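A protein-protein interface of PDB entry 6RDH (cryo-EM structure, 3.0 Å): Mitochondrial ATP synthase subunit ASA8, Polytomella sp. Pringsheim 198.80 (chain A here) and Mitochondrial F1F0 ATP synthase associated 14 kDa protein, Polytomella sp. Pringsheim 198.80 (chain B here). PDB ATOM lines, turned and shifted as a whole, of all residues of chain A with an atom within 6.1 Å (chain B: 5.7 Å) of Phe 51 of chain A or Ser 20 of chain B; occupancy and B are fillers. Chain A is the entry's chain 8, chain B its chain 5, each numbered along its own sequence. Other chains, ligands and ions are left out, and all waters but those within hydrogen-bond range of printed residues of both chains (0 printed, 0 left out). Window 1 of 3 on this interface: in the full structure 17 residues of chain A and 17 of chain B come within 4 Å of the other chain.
The backbone carbonyl oxygen of Ala 16 of chain B sits close to the side-chain hydroxyl of Ser 20 of chain B, 3.0 Å away.
Among the printed residues, pairs that only touch across the chains: Leu 47 of chain A with Leu 23 of chain B (3.8 Å), Phe 51 of chain A with Ala 16 of chain B (3.7 Å), Phe 51 of chain A with Ala 19 of chain B (3.6 Å), Phe 51 of chain A with Ser 20 of chain B (3.5 Å) and Ile 55 of chain A with Ala 16 of chain B (3.8 Å).
Printed residues of chain B within 4 Å of Leu 47 of chain A: Leu 23.
Of chain B, only Ala 16, Ala 19 and Ser 20 come within 4 Å of Phe 51 of chain A.
Printed residues of chain B within 4 Å of Ile 55 of chain A: Ala 16.
Printed residues of chain A within 4 Å of Ala 16 of chain B: Phe 51 and Ile 55.
Printed residues of chain A within 4 Å of Ala 19 of chain B: Phe 51 (3.6 Å).
Of chain A, only Phe 51 comes within 4 Å of Ser 20 of chain B.
Of the printed residues of chain A, Leu 23 of chain B touches Leu 47.
Trp 24 of chain B touches none of the printed residues of chain A.
The nearest residue of chain B that does not touch Phe 51 of chain A is Ala 15 of chain B (4.6 Å).
Hydrophobic or aromatic side chains of chain A that line the printed part of chain B: Leu 47, Phe 51 and Ile 55.
Along chain A the printed residues that touch a printed residue of chain B span positions 47 to 55.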
ATOM      1  N   TYR A  46      -5.504 -15.599  -4.639  1.00  0.00           N
ATOM      2  CA  TYR A  46      -5.381 -15.453  -3.195  1.00  0.00           C
ATOM      3  C   TYR A  46      -5.642 -16.773  -2.484  1.00  0.00           C
ATOM      4  O   TYR A  46      -4.913 -17.130  -1.558  1.00  0.00           O
ATOM      5  CB  TYR A  46      -6.344 -14.392  -2.687  1.00  0.00           C
ATOM      6  CG  TYR A  46      -6.449 -13.163  -3.540  1.00  0.00           C
ATOM      7  CD1 TYR A  46      -5.599 -12.098  -3.351  1.00  0.00           C
ATOM      8  CD2 TYR A  46      -7.430 -13.048  -4.499  1.00  0.00           C
ATOM      9  CE1 TYR A  46      -5.707 -10.967  -4.113  1.00  0.00           C
ATOM     10  CE2 TYR A  46      -7.538 -11.932  -5.270  1.00  0.00           C
ATOM     11  CZ  TYR A  46      -6.677 -10.895  -5.074  1.00  0.00           C
ATOM     12  OH  TYR A  46      -6.797  -9.772  -5.850  1.00  0.00           O
ATOM     13  N   LEU A  47      -6.669 -17.517  -2.909  1.00  0.00           N
ATOM     14  CA  LEU A  47      -6.908 -18.838  -2.336  1.00  0.00           C
ATOM     15  C   LEU A  47      -5.804 -19.814  -2.682  1.00  0.00           C
ATOM     16  O   LEU A  47      -5.426 -20.641  -1.850  1.00  0.00           O
ATOM     17  CB  LEU A  47      -8.231 -19.424  -2.799  1.00  0.00           C
ATOM     18  CG  LEU A  47      -9.443 -19.363  -1.893  1.00  0.00           C
ATOM     19  CD1 LEU A  47     -10.419 -20.383  -2.389  1.00  0.00           C
ATOM     20  CD2 LEU A  47      -9.060 -19.675  -0.480  1.00  0.00           C
ATOM     21  N   LEU A  48      -5.286 -19.754  -3.905  1.00  0.00           N
ATOM     22  CA  LEU A  48      -4.214 -20.678  -4.260  1.00  0.00           C
ATOM     23  C   LEU A  48      -2.926 -20.340  -3.521  1.00  0.00           C
ATOM     24  O   LEU A  48      -2.191 -21.240  -3.104  1.00  0.00           O
ATOM     25  CB  LEU A  48      -3.994 -20.676  -5.764  1.00  0.00           C
ATOM     26  CG  LEU A  48      -5.199 -21.106  -6.592  1.00  0.00           C
ATOM     27  CD1 LEU A  48      -4.807 -21.143  -8.041  1.00  0.00           C
ATOM     28  CD2 LEU A  48      -5.737 -22.440  -6.143  1.00  0.00           C
ATOM     29  N   GLY A  49      -2.660 -19.052  -3.299  1.00  0.00           N
ATOM     30  CA  GLY A  49      -1.541 -18.663  -2.466  1.00  0.00           C
ATOM     31  C   GLY A  49      -1.722 -19.045  -1.016  1.00  0.00           C
ATOM     32  O   GLY A  49      -0.753 -19.397  -0.347  1.00  0.00           O
ATOM     33  N   GLY A  50      -2.958 -19.010  -0.520  1.00  0.00           N
ATOM     34  CA  GLY A  50      -3.212 -19.473   0.832  1.00  0.00           C
ATOM     35  C   GLY A  50      -3.011 -20.966   0.996  1.00  0.00           C
ATOM     36  O   GLY A  50      -2.438 -21.419   1.991  1.00  0.00           O
ATOM     37  N   PHE A  51      -3.460 -21.748   0.018  1.00  0.00           N
ATOM     38  CA  PHE A  51      -3.262 -23.191   0.071  1.00  0.00           C
ATOM     39  C   PHE A  51      -1.789 -23.553  -0.051  1.00  0.00           C
ATOM     40  O   PHE A  51      -1.311 -24.448   0.653  1.00  0.00           O
ATOM     41  CB  PHE A  51      -4.079 -23.874  -1.021  1.00  0.00           C
ATOM     42  CG  PHE A  51      -5.546 -23.906  -0.739  1.00  0.00           C
ATOM     43  CD1 PHE A  51      -6.006 -24.217   0.519  1.00  0.00           C
ATOM     44  CD2 PHE A  51      -6.463 -23.619  -1.723  1.00  0.00           C
ATOM     45  CE1 PHE A  51      -7.351 -24.234   0.794  1.00  0.00           C
ATOM     46  CE2 PHE A  51      -7.805 -23.636  -1.455  1.00  0.00           C
ATOM     47  CZ  PHE A  51      -8.246 -23.943  -0.195  1.00  0.00           C
ATOM     48  N   THR A  52      -1.039 -22.844  -0.897  1.00  0.00           N
ATOM     49  CA  THR A  52       0.389 -23.126  -0.980  1.00  0.00           C
ATOM     50  C   THR A  52       1.138 -22.669   0.259  1.00  0.00           C
ATOM     51  O   THR A  52       2.102 -23.331   0.659  1.00  0.00           O
ATOM     52  CB  THR A  52       1.006 -22.487  -2.212  1.00  0.00           C
ATOM     53  OG1 THR A  52       0.741 -21.083  -2.207  1.00  0.00           O
ATOM     54  CG2 THR A  52       0.457 -23.126  -3.465  1.00  0.00           C
ATOM     55  N   PHE A  53       0.716 -21.567   0.886  1.00  0.00           N
ATOM     56  CA  PHE A  53       1.330 -21.157   2.142  1.00  0.00           C
ATOM     57  C   PHE A  53       1.107 -22.198   3.223  1.00  0.00           C
ATOM     58  O   PHE A  53       2.025 -22.507   3.985  1.00  0.00           O
ATOM     59  CB  PHE A  53       0.781 -19.813   2.605  1.00  0.00           C
ATOM     60  CG  PHE A  53       1.256 -19.410   3.974  1.00  0.00           C
ATOM     61  CD1 PHE A  53       2.525 -18.911   4.152  1.00  0.00           C
ATOM     62  CD2 PHE A  53       0.435 -19.533   5.081  1.00  0.00           C
ATOM     63  CE1 PHE A  53       2.967 -18.546   5.397  1.00  0.00           C
ATOM     64  CE2 PHE A  53       0.877 -19.169   6.327  1.00  0.00           C
ATOM     65  CZ  PHE A  53       2.140 -18.674   6.483  1.00  0.00           C
ATOM     66  N   THR A  54      -0.101 -22.750   3.301  1.00  0.00           N
ATOM     67  CA  THR A  54      -0.368 -23.759   4.316  1.00  0.00           C
ATOM     68  C   THR A  54       0.409 -25.037   4.051  1.00  0.00           C
ATOM     69  O   THR A  54       0.913 -25.657   4.990  1.00  0.00           O
ATOM     70  CB  THR A  54      -1.852 -24.055   4.380  1.00  0.00           C
ATOM     71  OG1 THR A  54      -2.558 -22.820   4.340  1.00  0.00           O
ATOM     72  CG2 THR A  54      -2.177 -24.734   5.653  1.00  0.00           C
ATOM     73  N   ILE A  55       0.552 -25.428   2.786  1.00  0.00           N
ATOM     74  CA  ILE A  55       1.288 -26.651   2.486  1.00  0.00           C
ATOM     75  C   ILE A  55       2.777 -26.482   2.783  1.00  0.00           C
ATOM     76  O   ILE A  55       3.406 -27.376   3.363  1.00  0.00           O
ATOM     77  CB  ILE A  55       1.013 -27.073   1.036  1.00  0.00           C
ATOM     78  CG1 ILE A  55      -0.426 -27.541   0.926  1.00  0.00           C
ATOM     79  CG2 ILE A  55       1.904 -28.197   0.615  1.00  0.00           C
ATOM     80  CD1 ILE A  55      -0.923 -27.624  -0.469  1.00  0.00           C
ATOM     81  N   THR A  56       3.346 -25.307   2.490  1.00  0.00           N
ATOM     82  CA  THR A  56       4.752 -25.086   2.829  1.00  0.00           C
ATOM     83  C   THR A  56       4.963 -24.952   4.332  1.00  0.00           C
ATOM     84  O   THR A  56       5.957 -25.457   4.861  1.00  0.00           O
ATOM     85  CB  THR A  56       5.298 -23.858   2.120  1.00  0.00           C
ATOM     86  OG1 THR A  56       4.522 -22.716   2.478  1.00  0.00           O
ATOM     87  CG2 THR A  56       5.265 -24.055   0.625  1.00  0.00           C
ATOM     88  N   ALA B  15      -6.606 -31.224   2.352  1.00  0.00           N
ATOM     89  CA  ALA B  15      -7.554 -30.127   2.511  1.00  0.00           C
ATOM     90  C   ALA B  15      -7.499 -29.168   1.335  1.00  0.00           C
ATOM     91  O   ALA B  15      -8.538 -28.709   0.852  1.00  0.00           O
ATOM     92  CB  ALA B  15      -7.276 -29.375   3.803  1.00  0.00           C
ATOM     93  N   ALA B  16      -6.296 -28.880   0.841  1.00  0.00           N
ATOM     94  CA  ALA B  16      -6.149 -27.977  -0.294  1.00  0.00           C
ATOM     95  C   ALA B  16      -6.678 -28.595  -1.578  1.00  0.00           C
ATOM     96  O   ALA B  16      -7.299 -27.904  -2.382  1.00  0.00           O
ATOM     97  CB  ALA B  16      -4.688 -27.583  -0.461  1.00  0.00           C
ATOM     98  N   VAL B  17      -6.469 -29.896  -1.772  1.00  0.00           N
ATOM     99  CA  VAL B  17      -6.967 -30.576  -2.964  1.00  0.00           C
ATOM    100  C   VAL B  17      -8.485 -30.642  -2.948  1.00  0.00           C
ATOM    101  O   VAL B  17      -9.138 -30.349  -3.952  1.00  0.00           O
ATOM    102  CB  VAL B  17      -6.333 -31.972  -3.077  1.00  0.00           C
ATOM    103  CG1 VAL B  17      -7.130 -32.871  -3.979  1.00  0.00           C
ATOM    104  CG2 VAL B  17      -4.944 -31.845  -3.612  1.00  0.00           C
ATOM    105  N   VAL B  18      -9.070 -30.965  -1.794  1.00  0.00           N
ATOM    106  CA  VAL B  18     -10.522 -31.081  -1.699  1.00  0.00           C
ATOM    107  C   VAL B  18     -11.185 -29.718  -1.858  1.00  0.00           C
ATOM    108  O   VAL B  18     -12.137 -29.571  -2.627  1.00  0.00           O
ATOM    109  CB  VAL B  18     -10.910 -31.757  -0.378  1.00  0.00           C
ATOM    110  CG1 VAL B  18     -12.362 -31.581  -0.095  1.00  0.00           C
ATOM    111  CG2 VAL B  18     -10.595 -33.214  -0.454  1.00  0.00           C
ATOM    112  N   ALA B  19     -10.664 -28.691  -1.187  1.00  0.00           N
ATOM    113  CA  ALA B  19     -11.278 -27.377  -1.308  1.00  0.00           C
ATOM    114  C   ALA B  19     -11.010 -26.737  -2.662  1.00  0.00           C
ATOM    115  O   ALA B  19     -11.851 -25.987  -3.160  1.00  0.00           O
ATOM    116  CB  ALA B  19     -10.801 -26.475  -0.186  1.00  0.00           C
ATOM    117  N   SER B  20      -9.886 -27.053  -3.306  1.00  0.00           N
ATOM    118  CA  SER B  20      -9.648 -26.542  -4.645  1.00  0.00           C
ATOM    119  C   SER B  20     -10.523 -27.235  -5.669  1.00  0.00           C
ATOM    120  O   SER B  20     -10.969 -26.599  -6.625  1.00  0.00           O
ATOM    121  CB  SER B  20      -8.186 -26.712  -5.013  1.00  0.00           C
ATOM    122  OG  SER B  20      -7.409 -25.682  -4.446  1.00  0.00           O
ATOM    123  N   TRP B  21     -10.803 -28.524  -5.481  1.00  0.00           N
ATOM    124  CA  TRP B  21     -11.744 -29.193  -6.363  1.00  0.00           C
ATOM    125  C   TRP B  21     -13.153 -28.682  -6.157  1.00  0.00           C
ATOM    126  O   TRP B  21     -13.909 -28.575  -7.118  1.00  0.00           O
ATOM    127  CB  TRP B  21     -11.718 -30.697  -6.151  1.00  0.00           C
ATOM    128  CG  TRP B  21     -12.617 -31.431  -7.082  1.00  0.00           C
ATOM    129  CD1 TRP B  21     -12.293 -31.915  -8.298  1.00  0.00           C
ATOM    130  CD2 TRP B  21     -13.991 -31.761  -6.874  1.00  0.00           C
ATOM    131  NE1 TRP B  21     -13.370 -32.527  -8.865  1.00  0.00           N
ATOM    132  CE2 TRP B  21     -14.429 -32.442  -8.006  1.00  0.00           C
ATOM    133  CE3 TRP B  21     -14.893 -31.541  -5.837  1.00  0.00           C
ATOM    134  CZ2 TRP B  21     -15.718 -32.907  -8.132  1.00  0.00           C
ATOM    135  CZ3 TRP B  21     -16.166 -31.998  -5.967  1.00  0.00           C
ATOM    136  CH2 TRP B  21     -16.569 -32.676  -7.102  1.00  0.00           C
ATOM    137  N   VAL B  22     -13.546 -28.410  -4.913  1.00  0.00           N
ATOM    138  CA  VAL B  22     -14.882 -27.877  -4.669  1.00  0.00           C
ATOM    139  C   VAL B  22     -15.003 -26.480  -5.250  1.00  0.00           C
ATOM    140  O   VAL B  22     -16.038 -26.130  -5.822  1.00  0.00           O
ATOM    141  CB  VAL B  22     -15.200 -27.926  -3.167  1.00  0.00           C
ATOM    142  CG1 VAL B  22     -16.436 -27.164  -2.840  1.00  0.00           C
ATOM    143  CG2 VAL B  22     -15.404 -29.345  -2.745  1.00  0.00           C
ATOM    144  N   LEU B  23     -13.926 -25.698  -5.210  1.00  0.00           N
ATOM    145  CA  LEU B  23     -13.924 -24.392  -5.855  1.00  0.00           C
ATOM    146  C   LEU B  23     -14.029 -24.507  -7.366  1.00  0.00           C
ATOM    147  O   LEU B  23     -14.798 -23.770  -7.986  1.00  0.00           O
ATOM    148  CB  LEU B  23     -12.663 -23.633  -5.481  1.00  0.00           C
ATOM    149  CG  LEU B  23     -12.469 -22.301  -6.169  1.00  0.00           C
ATOM    150  CD1 LEU B  23     -13.542 -21.376  -5.717  1.00  0.00           C
ATOM    151  CD2 LEU B  23     -11.125 -21.770  -5.805  1.00  0.00           C
ATOM    152  N   TRP B  24     -13.275 -25.425  -7.973  1.00  0.00           N
ATOM    153  CA  TRP B  24     -13.362 -25.610  -9.418  1.00  0.00           C
ATOM    154  C   TRP B  24     -14.734 -26.118  -9.823  1.00  0.00           C
ATOM    155  O   TRP B  24     -15.298 -25.650 -10.811  1.00  0.00           O
ATOM    156  CB  TRP B  24     -12.291 -26.578  -9.915  1.00  0.00           C
ATOM    157  CG  TRP B  24     -12.542 -27.073 -11.312  1.00  0.00           C
ATOM    158  CD1 TRP B  24     -12.177 -26.467 -12.463  1.00  0.00           C
ATOM    159  CD2 TRP B  24     -13.214 -28.277 -11.693  1.00  0.00           C
ATOM    160  NE1 TRP B  24     -12.583 -27.206 -13.542  1.00  0.00           N
ATOM    161  CE2 TRP B  24     -13.228 -28.323 -13.090  1.00  0.00           C
ATOM    162  CE3 TRP B  24     -13.814 -29.312 -10.984  1.00  0.00           C
ATOM    163  CZ2 TRP B  24     -13.811 -29.361 -13.785  1.00  0.00           C
ATOM    164  CZ3 TRP B  24     -14.396 -30.329 -11.672  1.00  0.00           C
ATOM    165  CH2 TRP B  24     -14.387 -30.356 -13.056  1.00  0.00           C
ATOM    166  N   HIS B  25     -15.290 -27.063  -9.069  1.00  0.00           N
ATOM    167  CA  HIS B  25     -16.552 -27.666  -9.459  1.00  0.00           C
ATOM    168  C   HIS B  25     -17.692 -26.696  -9.291  1.00  0.00           C
ATOM    169  O   HIS B  25     -18.563 -26.629 -10.153  1.00  0.00           O
ATOM    170  CB  HIS B  25     -16.819 -28.922  -8.658  1.00  0.00           C
ATOM    171  CG  HIS B  25     -17.987 -29.700  -9.157  1.00  0.00           C
ATOM    172  ND1 HIS B  25     -19.216 -29.672  -8.542  1.00  0.00           N
ATOM    173  CD2 HIS B  25     -18.124 -30.506 -10.232  1.00  0.00           C
ATOM    174  CE1 HIS B  25     -20.055 -30.439  -9.208  1.00  0.00           C
ATOM    175  NE2 HIS B  25     -19.416 -30.957 -10.239  1.00  0.00           N
